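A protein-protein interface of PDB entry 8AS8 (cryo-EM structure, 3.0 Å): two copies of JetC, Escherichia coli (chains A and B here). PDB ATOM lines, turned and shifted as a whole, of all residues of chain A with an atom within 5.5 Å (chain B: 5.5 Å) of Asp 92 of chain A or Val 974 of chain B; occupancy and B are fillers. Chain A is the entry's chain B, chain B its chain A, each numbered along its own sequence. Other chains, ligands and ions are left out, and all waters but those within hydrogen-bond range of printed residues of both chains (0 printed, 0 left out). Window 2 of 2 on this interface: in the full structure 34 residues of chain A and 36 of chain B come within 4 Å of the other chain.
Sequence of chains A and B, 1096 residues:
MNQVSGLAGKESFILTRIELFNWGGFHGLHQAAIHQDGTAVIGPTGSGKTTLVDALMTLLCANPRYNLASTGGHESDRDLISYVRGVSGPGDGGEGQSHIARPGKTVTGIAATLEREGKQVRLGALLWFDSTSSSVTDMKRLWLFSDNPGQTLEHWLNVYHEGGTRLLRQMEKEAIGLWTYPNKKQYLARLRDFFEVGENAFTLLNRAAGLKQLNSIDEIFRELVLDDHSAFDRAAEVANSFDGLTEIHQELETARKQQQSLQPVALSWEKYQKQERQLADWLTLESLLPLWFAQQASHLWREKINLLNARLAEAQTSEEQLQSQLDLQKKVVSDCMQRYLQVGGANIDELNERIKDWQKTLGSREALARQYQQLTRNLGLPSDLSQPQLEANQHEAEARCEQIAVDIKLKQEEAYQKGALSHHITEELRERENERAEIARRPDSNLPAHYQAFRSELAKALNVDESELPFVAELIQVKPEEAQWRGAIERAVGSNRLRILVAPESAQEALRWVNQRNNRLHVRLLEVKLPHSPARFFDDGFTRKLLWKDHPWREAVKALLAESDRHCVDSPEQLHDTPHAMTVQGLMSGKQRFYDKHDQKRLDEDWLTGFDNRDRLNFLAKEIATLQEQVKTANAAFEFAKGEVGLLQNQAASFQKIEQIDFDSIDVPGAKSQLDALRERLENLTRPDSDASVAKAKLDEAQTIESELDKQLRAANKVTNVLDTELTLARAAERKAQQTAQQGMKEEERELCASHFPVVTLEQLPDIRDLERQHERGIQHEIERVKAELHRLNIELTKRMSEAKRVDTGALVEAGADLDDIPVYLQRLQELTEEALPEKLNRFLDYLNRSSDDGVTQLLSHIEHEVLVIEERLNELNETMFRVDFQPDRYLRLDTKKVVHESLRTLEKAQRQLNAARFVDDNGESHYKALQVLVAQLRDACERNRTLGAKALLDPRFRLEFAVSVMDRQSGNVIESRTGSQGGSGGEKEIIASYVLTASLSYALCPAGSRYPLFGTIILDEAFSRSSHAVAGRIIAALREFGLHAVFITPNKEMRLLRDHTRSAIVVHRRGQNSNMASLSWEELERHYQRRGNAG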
ATOM      1  N   PRO A  90      16.549 -22.922 -19.892  1.00  0.00           N
ATOM      2  CA  PRO A  90      15.991 -24.084 -19.194  1.00  0.00           C
ATOM      3  C   PRO A  90      16.321 -24.085 -17.694  1.00  0.00           C
ATOM      4  O   PRO A  90      15.416 -24.308 -16.910  1.00  0.00           O
ATOM      5  CB  PRO A  90      16.622 -25.300 -19.891  1.00  0.00           C
ATOM      6  CG  PRO A  90      17.559 -24.730 -20.942  1.00  0.00           C
ATOM      7  CD  PRO A  90      17.118 -23.300 -21.179  1.00  0.00           C
ATOM      8  N   GLY A  91      17.585 -23.839 -17.329  1.00  0.00           N
ATOM      9  CA  GLY A  91      17.925 -23.767 -15.924  1.00  0.00           C
ATOM     10  C   GLY A  91      18.682 -24.960 -15.383  1.00  0.00           C
ATOM     11  O   GLY A  91      18.325 -25.504 -14.334  1.00  0.00           O
ATOM     12  N   ASP A  92      19.731 -25.380 -16.087  1.00  0.00           N
ATOM     13  CA  ASP A  92      20.582 -26.455 -15.594  1.00  0.00           C
ATOM     14  C   ASP A  92      19.781 -27.741 -15.441  1.00  0.00           C
ATOM     15  O   ASP A  92      18.666 -27.849 -15.963  1.00  0.00           O
ATOM     16  CB  ASP A  92      21.219 -26.049 -14.263  1.00  0.00           C
ATOM     17  CG  ASP A  92      22.415 -26.901 -13.900  1.00  0.00           C
ATOM     18  OD1 ASP A  92      22.232 -28.116 -13.675  1.00  0.00           O
ATOM     19  OD2 ASP A  92      23.535 -26.355 -13.834  1.00  0.00           O
ATOM     20  N   GLY A  93      20.331 -28.718 -14.727  1.00  0.00           N
ATOM     21  CA  GLY A  93      19.651 -29.982 -14.530  1.00  0.00           C
ATOM     22  C   GLY A  93      19.580 -30.398 -13.075  1.00  0.00           C
ATOM     23  O   GLY A  93      19.106 -31.492 -12.756  1.00  0.00           O
ATOM     24  N   GLY A  94      20.050 -29.530 -12.185  1.00  0.00           N
ATOM     25  CA  GLY A  94      20.030 -29.816 -10.764  1.00  0.00           C
ATOM     26  C   GLY A  94      19.287 -28.769  -9.963  1.00  0.00           C
ATOM     27  O   GLY A  94      19.702 -28.410  -8.857  1.00  0.00           O
ATOM     28  N   GLU A  95      18.181 -28.272 -10.513  1.00  0.00           N
ATOM     29  CA  GLU A  95      17.408 -27.222  -9.862  1.00  0.00           C
ATOM     30  C   GLU A  95      18.256 -25.970  -9.684  1.00  0.00           C
ATOM     31  O   GLU A  95      18.682 -25.357 -10.669  1.00  0.00           O
ATOM     32  CB  GLU A  95      16.878 -27.704  -8.510  1.00  0.00           C
ATOM     33  CG  GLU A  95      15.932 -28.888  -8.606  1.00  0.00           C
ATOM     34  CD  GLU A  95      16.660 -30.217  -8.622  1.00  0.00           C
ATOM     35  OE1 GLU A  95      17.097 -30.668  -7.543  1.00  0.00           O
ATOM     36  OE2 GLU A  95      16.798 -30.808  -9.713  1.00  0.00           O
ATOM     37  N   HIS A  99      18.540 -19.874 -12.902  1.00  0.00           N
ATOM     38  CA  HIS A  99      17.964 -19.324 -14.124  1.00  0.00           C
ATOM     39  C   HIS A  99      16.805 -18.387 -13.814  1.00  0.00           C
ATOM     40  O   HIS A  99      16.692 -17.310 -14.408  1.00  0.00           O
ATOM     41  CB  HIS A  99      17.508 -20.455 -15.042  1.00  0.00           C
ATOM     42  CG  HIS A  99      16.572 -21.423 -14.388  1.00  0.00           C
ATOM     43  ND1 HIS A  99      16.965 -22.269 -13.374  1.00  0.00           N
ATOM     44  CD2 HIS A  99      15.263 -21.687 -14.611  1.00  0.00           C
ATOM     45  CE1 HIS A  99      15.938 -23.007 -12.996  1.00  0.00           C
ATOM     46  NE2 HIS A  99      14.893 -22.674 -13.732  1.00  0.00           N
ATOM     47  N   ARG B 893      27.548 -31.499 -24.770  1.00  0.00           N
ATOM     48  CA  ARG B 893      27.265 -32.928 -24.757  1.00  0.00           C
ATOM     49  C   ARG B 893      25.781 -33.143 -25.019  1.00  0.00           C
ATOM     50  O   ARG B 893      24.986 -32.201 -25.003  1.00  0.00           O
ATOM     51  CB  ARG B 893      27.662 -33.570 -23.421  1.00  0.00           C
ATOM     52  CG  ARG B 893      27.677 -35.086 -23.446  1.00  0.00           C
ATOM     53  CD  ARG B 893      27.383 -35.685 -22.084  1.00  0.00           C
ATOM     54  NE  ARG B 893      26.134 -35.182 -21.527  1.00  0.00           N
ATOM     55  CZ  ARG B 893      25.835 -35.184 -20.236  1.00  0.00           C
ATOM     56  NH1 ARG B 893      26.676 -35.660 -19.332  1.00  0.00           N
ATOM     57  NH2 ARG B 893      24.661 -34.699 -19.840  1.00  0.00           N
ATOM     58  N   SER B 965      23.480 -30.133 -23.652  1.00  0.00           N
ATOM     59  CA  SER B 965      23.922 -29.645 -22.351  1.00  0.00           C
ATOM     60  C   SER B 965      25.309 -29.045 -22.517  1.00  0.00           C
ATOM     61  O   SER B 965      26.257 -29.758 -22.853  1.00  0.00           O
ATOM     62  CB  SER B 965      23.929 -30.767 -21.319  1.00  0.00           C
ATOM     63  OG  SER B 965      22.648 -31.358 -21.206  1.00  0.00           O
ATOM     64  N   VAL B 966      25.422 -27.743 -22.297  1.00  0.00           N
ATOM     65  CA  VAL B 966      26.722 -27.089 -22.275  1.00  0.00           C
ATOM     66  C   VAL B 966      27.304 -27.220 -20.875  1.00  0.00           C
ATOM     67  O   VAL B 966      26.647 -26.890 -19.879  1.00  0.00           O
ATOM     68  CB  VAL B 966      26.604 -25.619 -22.703  1.00  0.00           C
ATOM     69  CG1 VAL B 966      25.681 -24.871 -21.772  1.00  0.00           C
ATOM     70  CG2 VAL B 966      27.973 -24.968 -22.733  1.00  0.00           C
ATOM     71  N   MET B 967      28.531 -27.721 -20.800  1.00  0.00           N
ATOM     72  CA  MET B 967      29.224 -28.001 -19.551  1.00  0.00           C
ATOM     73  C   MET B 967      30.503 -27.170 -19.476  1.00  0.00           C
ATOM     74  O   MET B 967      30.743 -26.280 -20.296  1.00  0.00           O
ATOM     75  CB  MET B 967      29.529 -29.494 -19.430  1.00  0.00           C
ATOM     76  CG  MET B 967      28.452 -30.398 -19.984  1.00  0.00           C
ATOM     77  SD  MET B 967      28.808 -32.128 -19.638  1.00  0.00           S
ATOM     78  CE  MET B 967      27.242 -32.662 -18.962  1.00  0.00           C
ATOM     79  N   GLY B 972      33.030 -30.886 -14.686  1.00  0.00           N
ATOM     80  CA  GLY B 972      32.112 -31.704 -15.456  1.00  0.00           C
ATOM     81  C   GLY B 972      30.651 -31.443 -15.167  1.00  0.00           C
ATOM     82  O   GLY B 972      29.794 -31.995 -15.866  1.00  0.00           O
ATOM     83  N   ASN B 973      30.348 -30.625 -14.165  1.00  0.00           N
ATOM     84  CA  ASN B 973      28.961 -30.347 -13.826  1.00  0.00           C
ATOM     85  C   ASN B 973      28.249 -29.686 -14.999  1.00  0.00           C
ATOM     86  O   ASN B 973      28.811 -28.831 -15.689  1.00  0.00           O
ATOM     87  CB  ASN B 973      28.886 -29.445 -12.594  1.00  0.00           C
ATOM     88  CG  ASN B 973      30.030 -29.681 -11.632  1.00  0.00           C
ATOM     89  OD1 ASN B 973      31.080 -29.048 -11.732  1.00  0.00           O
ATOM     90  ND2 ASN B 973      29.833 -30.596 -10.690  1.00  0.00           N
ATOM     91  N   VAL B 974      27.000 -30.091 -15.222  1.00  0.00           N
ATOM     92  CA  VAL B 974      26.181 -29.448 -16.239  1.00  0.00           C
ATOM     93  C   VAL B 974      25.994 -27.985 -15.871  1.00  0.00           C
ATOM     94  O   VAL B 974      25.571 -27.659 -14.755  1.00  0.00           O
ATOM     95  CB  VAL B 974      24.828 -30.161 -16.370  1.00  0.00           C
ATOM     96  CG1 VAL B 974      23.765 -29.186 -16.842  1.00  0.00           C
ATOM     97  CG2 VAL B 974      24.939 -31.337 -17.319  1.00  0.00           C
ATOM     98  N   ILE B 975      26.314 -27.093 -16.804  1.00  0.00           N
ATOM     99  CA  ILE B 975      26.131 -25.667 -16.581  1.00  0.00           C
ATOM    100  C   ILE B 975      24.866 -25.137 -17.239  1.00  0.00           C
ATOM    101  O   ILE B 975      24.298 -24.152 -16.743  1.00  0.00           O
ATOM    102  CB  ILE B 975      27.355 -24.856 -17.052  1.00  0.00           C
ATOM    103  CG1 ILE B 975      27.214 -24.468 -18.522  1.00  0.00           C
ATOM    104  CG2 ILE B 975      28.629 -25.652 -16.839  1.00  0.00           C
ATOM    105  CD1 ILE B 975      26.613 -23.095 -18.736  1.00  0.00           C
ATOM    106  N   GLU B 976      24.407 -25.743 -18.332  1.00  0.00           N
ATOM    107  CA  GLU B 976      23.164 -25.304 -18.961  1.00  0.00           C
ATOM    108  C   GLU B 976      22.612 -26.467 -19.771  1.00  0.00           C
ATOM    109  O   GLU B 976      23.146 -26.779 -20.838  1.00  0.00           O
ATOM    110  CB  GLU B 976      23.413 -24.082 -19.835  1.00  0.00           C
ATOM    111  CG  GLU B 976      22.422 -23.878 -20.965  1.00  0.00           C
ATOM    112  CD  GLU B 976      20.998 -23.698 -20.484  1.00  0.00           C
ATOM    113  OE1 GLU B 976      20.641 -24.249 -19.423  1.00  0.00           O
ATOM    114  OE2 GLU B 976      20.239 -22.986 -21.172  1.00  0.00           O
ATOM    115  N   SER B 977      21.546 -27.094 -19.277  1.00  0.00           N
ATOM    116  CA  SER B 977      20.988 -28.296 -19.889  1.00  0.00           C
ATOM    117  C   SER B 977      19.634 -27.960 -20.495  1.00  0.00           C
ATOM    118  O   SER B 977      18.660 -27.739 -19.767  1.00  0.00           O
ATOM    119  CB  SER B 977      20.860 -29.421 -18.865  1.00  0.00           C
ATOM    120  OG  SER B 977      19.788 -29.173 -17.975  1.00  0.00           O
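Hydrophobic or aromatic side chains of chain B within 4 Å of the printed part of chain A: Val 974.
Printed residues of chain A that touch a printed residue of chain B: Pro 90, Gly 91, Asp 92 and Gly 93.
Hydrophobic or aromatic side chains of chain A within 4 Å of the printed part of chain B: Pro 90.
Among the printed residues, 8 pairs touch across the chains.
Among the printed residues, no Asp or Glu carboxylate lies within 4 Å of a Lys or Arg side-chain nitrogen of the other chain.
OD2 of Asp 92 of chain A sits close to O of Val 974 of chain B (2.6 Å).
The side-chain hydroxyl of Ser 977 of chain B lies within hydrogen-bond range of the backbone carbonyl oxygen of Asp 92 of chain A (2.7 Å).
The side-chain hydroxyl (OG) of Ser 977 of chain B lies within hydrogen-bond range of the backbone NH (N) of Gly 93 of chain A, at 3.3 Å.
No position is printed for both chains.
Of the printed residues of chain B, Pro 90 of chain A touches Glu 976 (3.1 Å) and Ser 977 (3.2 Å).
Of chain B, only Val 974 (2.6 Å), Ile 975 (3.7 Å), Glu 976 (3.6 Å) and Ser 977 (2.7 Å) come within 4 Å of Asp 92 of chain A.
Of the printed residues of chain B, Gly 93 of chain A touches Ser 977.
Val 974 of chain B touches just one residue of chain A: Asp 92 (2.6 Å).
Of the printed residues of chain A, Ile 975 of chain B touches Asp 92.
The nearest printed residue of chain A that does not touch Ser 977 of chain B is Gly 91 of chain A (4.7 Å).
Glu 976 of chain B touches Pro 90 of chain A.
Pro 90 of chain A touches Ser 977 of chain B (CB to O, 3.2 Å).
Gly 91 of chain A touches Glu 976 of chain B (N to OE1, 3.7 Å).
Asp 92 of chain A touches Ile 975 of chain B (OD2 to O, 3.7 Å).
N of Asp 92 of chain A touches OE1 of Glu 976 of chain B, at 3.6 Å.
N of Ile 975 of chain B sits close to O of Val 966 of chain B (3.1 Å).
The backbone carbonyl oxygen (O) of Glu 976 of chain B sits at hydrogen-bond distance from the backbone NH (N) of Val 966 of chain B, at 2.9 Å.
The backbone NH (N) of Gly 94 of chain A is in hydrogen-bond range of the side-chain carboxylate (OD1) of Asp 92 of chain A (3.0 Å).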
